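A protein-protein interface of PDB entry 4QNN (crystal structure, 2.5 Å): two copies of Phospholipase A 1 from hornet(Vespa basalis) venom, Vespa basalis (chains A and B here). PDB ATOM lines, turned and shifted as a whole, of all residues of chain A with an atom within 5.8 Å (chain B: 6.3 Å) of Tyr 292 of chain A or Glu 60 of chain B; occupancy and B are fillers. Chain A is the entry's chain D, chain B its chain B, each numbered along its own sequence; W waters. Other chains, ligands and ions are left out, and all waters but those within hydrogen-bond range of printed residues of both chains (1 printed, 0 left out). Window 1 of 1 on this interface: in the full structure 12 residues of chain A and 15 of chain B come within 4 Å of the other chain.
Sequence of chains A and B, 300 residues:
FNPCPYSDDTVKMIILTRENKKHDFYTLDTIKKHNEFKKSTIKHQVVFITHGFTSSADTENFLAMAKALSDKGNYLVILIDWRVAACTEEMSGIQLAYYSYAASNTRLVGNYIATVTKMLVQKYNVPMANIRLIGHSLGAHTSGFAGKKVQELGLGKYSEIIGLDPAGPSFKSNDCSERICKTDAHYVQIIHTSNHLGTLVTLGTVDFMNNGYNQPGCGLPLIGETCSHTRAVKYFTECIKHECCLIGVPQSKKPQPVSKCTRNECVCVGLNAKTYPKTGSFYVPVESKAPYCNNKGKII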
ATOM      1  N   PRO A 216       8.842 -12.385 -33.795  1.00  0.00           N
ATOM      2  CA  PRO A 216       9.465 -13.695 -33.604  1.00  0.00           C
ATOM      3  C   PRO A 216       8.535 -14.648 -32.845  1.00  0.00           C
ATOM      4  O   PRO A 216       7.983 -14.295 -31.796  1.00  0.00           O
ATOM      5  CB  PRO A 216      10.723 -13.363 -32.788  1.00  0.00           C
ATOM      6  CG  PRO A 216      11.015 -11.950 -33.157  1.00  0.00           C
ATOM      7  CD  PRO A 216       9.645 -11.340 -33.136  1.00  0.00           C
ATOM      8  N   GLY A 217       8.375 -15.850 -33.380  1.00  0.00           N
ATOM      9  CA  GLY A 217       7.525 -16.823 -32.731  1.00  0.00           C
ATOM     10  C   GLY A 217       6.094 -16.734 -33.187  1.00  0.00           C
ATOM     11  O   GLY A 217       5.253 -17.508 -32.728  1.00  0.00           O
ATOM     12  N   CYS A 218       5.810 -15.797 -34.090  1.00  0.00           N
ATOM     13  CA  CYS A 218       4.451 -15.641 -34.592  1.00  0.00           C
ATOM     14  C   CYS A 218       4.213 -16.406 -35.898  1.00  0.00           C
ATOM     15  O   CYS A 218       3.100 -16.421 -36.437  1.00  0.00           O
ATOM     16  CB  CYS A 218       4.103 -14.173 -34.796  1.00  0.00           C
ATOM     17  SG  CYS A 218       3.400 -13.262 -33.384  1.00  0.00           S
ATOM     18  N   ARG A 231       0.801  -9.006 -30.514  1.00  0.00           N
ATOM     19  CA  ARG A 231       2.007  -8.937 -29.676  1.00  0.00           C
ATOM     20  C   ARG A 231       2.208  -7.590 -28.955  1.00  0.00           C
ATOM     21  O   ARG A 231       2.761  -7.540 -27.855  1.00  0.00           O
ATOM     22  CB  ARG A 231       3.239  -9.200 -30.516  1.00  0.00           C
ATOM     23  CG  ARG A 231       3.557 -10.652 -30.731  1.00  0.00           C
ATOM     24  CD  ARG A 231       4.027 -11.262 -29.434  1.00  0.00           C
ATOM     25  NE  ARG A 231       4.288 -12.696 -29.543  1.00  0.00           N
ATOM     26  CZ  ARG A 231       5.432 -13.216 -29.954  1.00  0.00           C
ATOM     27  NH1 ARG A 231       6.420 -12.419 -30.299  1.00  0.00           N
ATOM     28  NH2 ARG A 231       5.587 -14.536 -29.998  1.00  0.00           N
ATOM     29  N   LYS A 234       0.569  -7.678 -25.647  1.00  0.00           N
ATOM     30  CA  LYS A 234       1.300  -8.498 -24.711  1.00  0.00           C
ATOM     31  C   LYS A 234       2.659  -7.891 -24.321  1.00  0.00           C
ATOM     32  O   LYS A 234       3.057  -7.927 -23.137  1.00  0.00           O
ATOM     33  CB  LYS A 234       1.463  -9.897 -25.300  1.00  0.00           C
ATOM     34  CG  LYS A 234       0.085 -10.540 -25.504  1.00  0.00           C
ATOM     35  CD  LYS A 234       0.103 -11.834 -26.304  1.00  0.00           C
ATOM     36  CE  LYS A 234       0.699 -13.011 -25.517  1.00  0.00           C
ATOM     37  NZ  LYS A 234       0.698 -14.214 -26.387  1.00  0.00           N
ATOM     38  N   TYR A 235       3.375  -7.320 -25.284  1.00  0.00           N
ATOM     39  CA  TYR A 235       4.660  -6.775 -24.933  1.00  0.00           C
ATOM     40  C   TYR A 235       4.504  -5.698 -23.859  1.00  0.00           C
ATOM     41  O   TYR A 235       5.240  -5.685 -22.871  1.00  0.00           O
ATOM     42  CB  TYR A 235       5.376  -6.175 -26.148  1.00  0.00           C
ATOM     43  CG  TYR A 235       5.842  -7.153 -27.204  1.00  0.00           C
ATOM     44  CD1 TYR A 235       6.343  -8.396 -26.866  1.00  0.00           C
ATOM     45  CD2 TYR A 235       5.795  -6.818 -28.552  1.00  0.00           C
ATOM     46  CE1 TYR A 235       6.790  -9.286 -27.843  1.00  0.00           C
ATOM     47  CE2 TYR A 235       6.242  -7.706 -29.551  1.00  0.00           C
ATOM     48  CZ  TYR A 235       6.741  -8.942 -29.182  1.00  0.00           C
ATOM     49  OH  TYR A 235       7.188  -9.829 -30.143  1.00  0.00           O
ATOM     50  N   GLU A 238       3.723  -7.058 -20.280  1.00  0.00           N
ATOM     51  CA  GLU A 238       4.925  -7.602 -19.688  1.00  0.00           C
ATOM     52  C   GLU A 238       5.847  -6.481 -19.224  1.00  0.00           C
ATOM     53  O   GLU A 238       6.630  -6.668 -18.275  1.00  0.00           O
ATOM     54  CB  GLU A 238       5.687  -8.472 -20.696  1.00  0.00           C
ATOM     55  CG  GLU A 238       4.932  -9.714 -21.174  1.00  0.00           C
ATOM     56  CD  GLU A 238       4.922 -10.876 -20.160  1.00  0.00           C
ATOM     57  OE1 GLU A 238       4.849 -10.618 -18.922  1.00  0.00           O
ATOM     58  OE2 GLU A 238       4.975 -12.053 -20.620  1.00  0.00           O
ATOM     59  N   CYS A 245      11.709  -4.672 -18.983  1.00  0.00           N
ATOM     60  CA  CYS A 245      11.619  -5.958 -19.650  1.00  0.00           C
ATOM     61  C   CYS A 245      12.120  -5.790 -21.074  1.00  0.00           C
ATOM     62  O   CYS A 245      12.820  -6.630 -21.642  1.00  0.00           O
ATOM     63  CB  CYS A 245      10.152  -6.390 -19.671  1.00  0.00           C
ATOM     64  SG  CYS A 245       9.748  -7.718 -20.853  1.00  0.00           S
ATOM     65  N   LEU A 246      11.733  -4.648 -21.627  1.00  0.00           N
ATOM     66  CA  LEU A 246      12.036  -4.271 -22.983  1.00  0.00           C
ATOM     67  C   LEU A 246      12.678  -2.909 -23.065  1.00  0.00           C
ATOM     68  O   LEU A 246      12.023  -1.885 -22.848  1.00  0.00           O
ATOM     69  CB  LEU A 246      10.755  -4.285 -23.801  1.00  0.00           C
ATOM     70  CG  LEU A 246      10.336  -5.700 -24.182  1.00  0.00           C
ATOM     71  CD1 LEU A 246       9.032  -5.660 -24.966  1.00  0.00           C
ATOM     72  CD2 LEU A 246      11.497  -6.364 -24.987  1.00  0.00           C
ATOM     73  N   PRO A 285      14.831  -5.192 -29.776  1.00  0.00           N
ATOM     74  CA  PRO A 285      14.973  -6.618 -30.052  1.00  0.00           C
ATOM     75  C   PRO A 285      14.045  -7.319 -29.093  1.00  0.00           C
ATOM     76  O   PRO A 285      13.804  -6.806 -28.030  1.00  0.00           O
ATOM     77  CB  PRO A 285      16.436  -6.874 -29.740  1.00  0.00           C
ATOM     78  CG  PRO A 285      16.702  -5.919 -28.637  1.00  0.00           C
ATOM     79  CD  PRO A 285      16.050  -4.668 -29.128  1.00  0.00           C
ATOM     80  N   VAL A 286      13.496  -8.461 -29.481  1.00  0.00           N
ATOM     81  CA  VAL A 286      12.575  -9.201 -28.616  1.00  0.00           C
ATOM     82  C   VAL A 286      12.819 -10.712 -28.698  1.00  0.00           C
ATOM     83  O   VAL A 286      13.434 -11.196 -29.649  1.00  0.00           O
ATOM     84  CB  VAL A 286      11.102  -8.904 -28.997  1.00  0.00           C
ATOM     85  CG1 VAL A 286      10.658  -7.603 -28.388  1.00  0.00           C
ATOM     86  CG2 VAL A 286      10.967  -8.830 -30.502  1.00  0.00           C
ATOM     87  N   GLU A 287      12.357 -11.449 -27.693  1.00  0.00           N
ATOM     88  CA  GLU A 287      12.502 -12.917 -27.681  1.00  0.00           C
ATOM     89  C   GLU A 287      11.196 -13.546 -28.201  1.00  0.00           C
ATOM     90  O   GLU A 287      10.170 -12.864 -28.255  1.00  0.00           O
ATOM     91  CB  GLU A 287      12.804 -13.427 -26.263  1.00  0.00           C
ATOM     92  CG  GLU A 287      14.235 -13.146 -25.779  1.00  0.00           C
ATOM     93  CD  GLU A 287      15.320 -13.654 -26.740  1.00  0.00           C
ATOM     94  OE1 GLU A 287      15.107 -14.689 -27.421  1.00  0.00           O
ATOM     95  OE2 GLU A 287      16.403 -13.026 -26.805  1.00  0.00           O
ATOM     96  N   SER A 288      11.230 -14.833 -28.556  1.00  0.00           N
ATOM     97  CA  SER A 288      10.078 -15.541 -29.124  1.00  0.00           C
ATOM     98  C   SER A 288       8.963 -16.075 -28.232  1.00  0.00           C
ATOM     99  O   SER A 288       7.969 -16.610 -28.750  1.00  0.00           O
ATOM    100  CB  SER A 288      10.560 -16.725 -29.955  1.00  0.00           C
ATOM    101  OG  SER A 288      11.382 -16.327 -31.032  1.00  0.00           O
ATOM    102  N   LYS A 289       9.104 -15.963 -26.919  1.00  0.00           N
ATOM    103  CA  LYS A 289       8.097 -16.504 -26.014  1.00  0.00           C
ATOM    104  C   LYS A 289       7.904 -15.577 -24.821  1.00  0.00           C
ATOM    105  O   LYS A 289       8.837 -14.908 -24.396  1.00  0.00           O
ATOM    106  CB  LYS A 289       8.560 -17.870 -25.495  1.00  0.00           C
ATOM    107  CG  LYS A 289       9.302 -18.751 -26.529  1.00  0.00           C
ATOM    108  CD  LYS A 289       9.962 -20.005 -25.899  1.00  0.00           C
ATOM    109  CE  LYS A 289      11.501 -19.904 -25.713  1.00  0.00           C
ATOM    110  NZ  LYS A 289      12.312 -20.151 -26.972  1.00  0.00           N
ATOM    111  N   ALA A 290       6.700 -15.533 -24.269  1.00  0.00           N
ATOM    112  CA  ALA A 290       6.481 -14.700 -23.103  1.00  0.00           C
ATOM    113  C   ALA A 290       7.603 -15.029 -22.123  1.00  0.00           C
ATOM    114  O   ALA A 290       7.972 -16.198 -21.969  1.00  0.00           O
ATOM    115  CB  ALA A 290       5.140 -15.007 -22.491  1.00  0.00           C
ATOM    116  N   PRO A 291       8.132 -14.017 -21.408  1.00  0.00           N
ATOM    117  CA  PRO A 291       7.745 -12.605 -21.447  1.00  0.00           C
ATOM    118  C   PRO A 291       8.503 -11.735 -22.471  1.00  0.00           C
ATOM    119  O   PRO A 291       8.532 -10.515 -22.363  1.00  0.00           O
ATOM    120  CB  PRO A 291       7.984 -12.175 -20.003  1.00  0.00           C
ATOM    121  CG  PRO A 291       9.268 -12.845 -19.710  1.00  0.00           C
ATOM    122  CD  PRO A 291       9.210 -14.213 -20.425  1.00  0.00           C
ATOM    123  N   TYR A 292       9.135 -12.363 -23.446  1.00  0.00           N
ATOM    124  CA  TYR A 292       9.831 -11.638 -24.489  1.00  0.00           C
ATOM    125  C   TYR A 292      10.950 -10.681 -24.095  1.00  0.00           C
ATOM    126  O   TYR A 292      11.710 -10.279 -24.966  1.00  0.00           O
ATOM    127  CB  TYR A 292       8.829 -10.838 -25.316  1.00  0.00           C
ATOM    128  CG  TYR A 292       7.534 -11.534 -25.631  1.00  0.00           C
ATOM    129  CD1 TYR A 292       7.454 -12.529 -26.609  1.00  0.00           C
ATOM    130  CD2 TYR A 292       6.382 -11.240 -24.901  1.00  0.00           C
ATOM    131  CE1 TYR A 292       6.246 -13.219 -26.838  1.00  0.00           C
ATOM    132  CE2 TYR A 292       5.182 -11.922 -25.120  1.00  0.00           C
ATOM    133  CZ  TYR A 292       5.120 -12.901 -26.081  1.00  0.00           C
ATOM    134  OH  TYR A 292       3.921 -13.539 -26.261  1.00  0.00           O
ATOM    135  N   CYS A 293      11.065 -10.307 -22.821  1.00  0.00           N
ATOM    136  CA  CYS A 293      12.095  -9.342 -22.395  1.00  0.00           C
ATOM    137  C   CYS A 293      13.449  -9.473 -23.081  1.00  0.00           C
ATOM    138  O   CYS A 293      13.884 -10.578 -23.381  1.00  0.00           O
ATOM    139  CB  CYS A 293      12.281  -9.396 -20.871  1.00  0.00           C
ATOM    140  SG  CYS A 293      10.683  -9.317 -20.012  1.00  0.00           S
ATOM    141  N   ASN A 294      14.116  -8.337 -23.305  1.00  0.00           N
ATOM    142  CA  ASN A 294      15.426  -8.310 -23.971  1.00  0.00           C
ATOM    143  C   ASN A 294      16.654  -8.018 -23.098  1.00  0.00           C
ATOM    144  O   ASN A 294      17.682  -7.657 -23.632  1.00  0.00           O
ATOM    145  CB  ASN A 294      15.424  -7.289 -25.132  1.00  0.00           C
ATOM    146  CG  ASN A 294      15.099  -5.852 -24.680  1.00  0.00           C
ATOM    147  OD1 ASN A 294      15.626  -5.358 -23.694  1.00  0.00           O
ATOM    148  ND2 ASN A 294      14.243  -5.190 -25.418  1.00  0.00           N
ATOM    149  N   ALA B  57       6.603 -25.413 -36.631  1.00  0.00           N
ATOM    150  CA  ALA B  57       7.302 -25.790 -35.430  1.00  0.00           C
ATOM    151  C   ALA B  57       7.858 -24.626 -34.650  1.00  0.00           C
ATOM    152  O   ALA B  57       7.950 -24.706 -33.436  1.00  0.00           O
ATOM    153  CB  ALA B  57       8.395 -26.739 -35.773  1.00  0.00           C
ATOM    154  N   ASP B  58       8.228 -23.538 -35.326  1.00  0.00           N
ATOM    155  CA  ASP B  58       8.790 -22.397 -34.619  1.00  0.00           C
ATOM    156  C   ASP B  58       7.817 -21.328 -34.178  1.00  0.00           C
ATOM    157  O   ASP B  58       8.119 -20.143 -34.297  1.00  0.00           O
ATOM    158  CB  ASP B  58       9.931 -21.723 -35.407  1.00  0.00           C
ATOM    159  CG  ASP B  58       9.743 -21.764 -36.916  1.00  0.00           C
ATOM    160  OD1 ASP B  58       8.613 -21.691 -37.459  1.00  0.00           O
ATOM    161  OD2 ASP B  58      10.786 -21.851 -37.578  1.00  0.00           O
ATOM    162  N   THR B  59       6.656 -21.731 -33.669  1.00  0.00           N
ATOM    163  CA  THR B  59       5.677 -20.763 -33.181  1.00  0.00           C
ATOM    164  C   THR B  59       5.923 -20.667 -31.685  1.00  0.00           C
ATOM    165  O   THR B  59       6.585 -21.530 -31.104  1.00  0.00           O
ATOM    166  CB  THR B  59       4.181 -21.186 -33.446  1.00  0.00           C
ATOM    167  OG1 THR B  59       3.707 -22.073 -32.416  1.00  0.00           O
ATOM    168  CG2 THR B  59       4.056 -21.862 -34.791  1.00  0.00           C
ATOM    169  N   GLU B  60       5.409 -19.614 -31.060  1.00  0.00           N
ATOM    170  CA  GLU B  60       5.630 -19.432 -29.632  1.00  0.00           C
ATOM    171  C   GLU B  60       5.202 -20.659 -28.835  1.00  0.00           C
ATOM    172  O   GLU B  60       6.027 -21.306 -28.205  1.00  0.00           O
ATOM    173  CB  GLU B  60       4.892 -18.191 -29.090  1.00  0.00           C
ATOM    174  CG  GLU B  60       5.401 -17.759 -27.717  1.00  0.00           C
ATOM    175  CD  GLU B  60       4.732 -16.499 -27.158  1.00  0.00           C
ATOM    176  OE1 GLU B  60       4.580 -15.509 -27.922  1.00  0.00           O
ATOM    177  OE2 GLU B  60       4.374 -16.500 -25.948  1.00  0.00           O
ATOM    178  N   ASN B  61       3.916 -20.974 -28.887  1.00  0.00           N
ATOM    179  CA  ASN B  61       3.366 -22.078 -28.142  1.00  0.00           C
ATOM    180  C   ASN B  61       4.122 -23.384 -28.228  1.00  0.00           C
ATOM    181  O   ASN B  61       4.409 -23.969 -27.201  1.00  0.00           O
ATOM    182  CB  ASN B  61       1.914 -22.243 -28.521  1.00  0.00           C
ATOM    183  CG  ASN B  61       1.124 -20.960 -28.295  1.00  0.00           C
ATOM    184  OD1 ASN B  61       1.263 -20.315 -27.258  1.00  0.00           O
ATOM    185  ND2 ASN B  61       0.289 -20.588 -29.264  1.00  0.00           N
ATOM    186  N   PHE B  62       4.481 -23.843 -29.418  1.00  0.00           N
ATOM    187  CA  PHE B  62       5.249 -25.079 -29.512  1.00  0.00           C
ATOM    188  C   PHE B  62       6.708 -24.935 -28.994  1.00  0.00           C
ATOM    189  O   PHE B  62       7.219 -25.849 -28.388  1.00  0.00           O
ATOM    190  CB  PHE B  62       5.223 -25.606 -30.945  1.00  0.00           C
ATOM    191  CG  PHE B  62       3.849 -25.962 -31.424  1.00  0.00           C
ATOM    192  CD1 PHE B  62       3.050 -26.853 -30.702  1.00  0.00           C
ATOM    193  CD2 PHE B  62       3.344 -25.425 -32.593  1.00  0.00           C
ATOM    194  CE1 PHE B  62       1.761 -27.203 -31.145  1.00  0.00           C
ATOM    195  CE2 PHE B  62       2.063 -25.767 -33.040  1.00  0.00           C
ATOM    196  CZ  PHE B  62       1.272 -26.658 -32.311  1.00  0.00           C
ATOM    197  N   LEU B  63       7.379 -23.812 -29.229  1.00  0.00           N
ATOM    198  CA  LEU B  63       8.734 -23.628 -28.711  1.00  0.00           C
ATOM    199  C   LEU B  63       8.743 -23.607 -27.182  1.00  0.00           C
ATOM    200  O   LEU B  63       9.653 -24.136 -26.562  1.00  0.00           O
ATOM    201  CB  LEU B  63       9.331 -22.318 -29.224  1.00  0.00           C
ATOM    202  CG  LEU B  63       9.571 -22.227 -30.727  1.00  0.00           C
ATOM    203  CD1 LEU B  63       9.874 -20.765 -31.089  1.00  0.00           C
ATOM    204  CD2 LEU B  63      10.716 -23.184 -31.150  1.00  0.00           C
ATOM    205  N   ALA B  64       7.734 -22.991 -26.572  1.00  0.00           N
ATOM    206  CA  ALA B  64       7.640 -22.948 -25.106  1.00  0.00           C
ATOM    207  C   ALA B  64       7.568 -24.375 -24.570  1.00  0.00           C
ATOM    208  O   ALA B  64       8.222 -24.717 -23.583  1.00  0.00           O
ATOM    209  CB  ALA B  64       6.393 -22.180 -24.661  1.00  0.00           C
ATOM    210  N   MET B  65       6.747 -25.200 -25.223  1.00  0.00           N
ATOM    211  CA  MET B  65       6.583 -26.580 -24.801  1.00  0.00           C
ATOM    212  C   MET B  65       7.924 -27.283 -24.916  1.00  0.00           C
ATOM    213  O   MET B  65       8.331 -28.007 -24.005  1.00  0.00           O
ATOM    214  CB  MET B  65       5.524 -27.292 -25.648  1.00  0.00           C
ATOM    215  CG  MET B  65       5.269 -28.763 -25.262  1.00  0.00           C
ATOM    216  SD  MET B  65       3.642 -29.392 -25.788  1.00  0.00           S
ATOM    217  CE  MET B  65       4.033 -29.926 -27.325  1.00  0.00           C
HETATM  218  O   HOH W   1       7.725 -17.549 -35.606  1.00  0.00           O
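Among the printed residues, pairs that only touch across the chains: Gly 217 of chain A with Asp 58 of chain B, Gly 217 of chain A with Thr 59 of chain B, Ser 288 of chain A with Glu 60 of chain B, Lys 289 of chain A with Glu 60 of chain B and Lys 289 of chain A with Ala 64 of chain B.
No position is printed for both chains.
The backbone NH (N) of Glu 60 of chain B sits at hydrogen-bond distance from the backbone carbonyl oxygen (O) of Gly 217 of chain A, at 2.7 Å.
The backbone NH of Ala 290 of chain A is in hydrogen-bond range of the side-chain carboxylate of Glu 60 of chain B.
The side-chain hydroxyl (OH) of Tyr 292 of chain A sits at hydrogen-bond distance from the side-chain carboxylate (OE1) of Glu 60 of chain B (2.7 Å).
The side-chain carboxylate (OE1) of Glu 60 of chain B is in salt-bridge range of the guanidinium group (NH2) of Arg 231 of chain A, 2.5 Å away.
The side-chain hydroxyl of Tyr 235 of chain A lies within hydrogen-bond range of the guanidinium group of Arg 231 of chain A, 2.7 Å away.
The backbone NH of Glu 287 of chain A sits at hydrogen-bond distance from the backbone carbonyl oxygen of Tyr 292 of chain A (3.0 Å).
OH of Tyr 292 of chain A sits close to NE of Arg 231 of chain A (3.4 Å).
The backbone carbonyl oxygen (O) of Ser 288 of chain A is in hydrogen-bond range of the guanidinium group (NH2) of Arg 231 of chain A, 3.4 Å away.
OH of Tyr 292 of chain A is in hydrogen-bond range of NZ of Lys 234 of chain A.
The side-chain sulfur (SG) of Cys 293 of chain A forms a disulfide with the side-chain sulfur (SG) of Cys 245 of chain A.
Of the printed residues of chain B, Gly 217 of chain A touches Asp 58, Thr 59 and Glu 60.
Of chain B, only Glu 60 (2.7 Å) comes within 4 Å of Tyr 292 of chain A.
Printed residues of chain A within 4 Å of Asp 58 of chain B: Gly 217 (3.7 Å).
Glu 60 of chain B touches just these residues of chain A: Gly 217 (2.7 Å), Arg 231 (2.5 Å), Ser 288 (3.0 Å), Lys 289 (3.4 Å), Ala 290 (3.0 Å) and Tyr 292 (2.7 Å).
The nearest printed residue of chain B that does not touch Tyr 292 of chain A is Asn 61 of chain B (7.3 Å).
The nearest residue of chain A that does not touch Glu 60 of chain B is Lys 234 of chain A (4.4 Å).
Hydrophobic or aromatic side chains of chain A within 4 Å of the printed part of chain B: Ala 290 and Tyr 292.
Along chain A the printed residues that touch a printed residue of chain B span positions 217 to 292.
Among the printed residues, Asp or Glu carboxylates within 4 Å of a Lys or Arg side-chain nitrogen of the other chain: Arg 231 of chain A with Glu 60 of chain B.
Water W1 lies within hydrogen-bond range of the backbone NH (N) of Gly 217 of chain A (2.9 Å), the backbone carbonyl oxygen (O) of Asp 58 of chain B (2.9 Å) and the backbone NH (N) of Cys 218 of chain A (3.0 Å).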
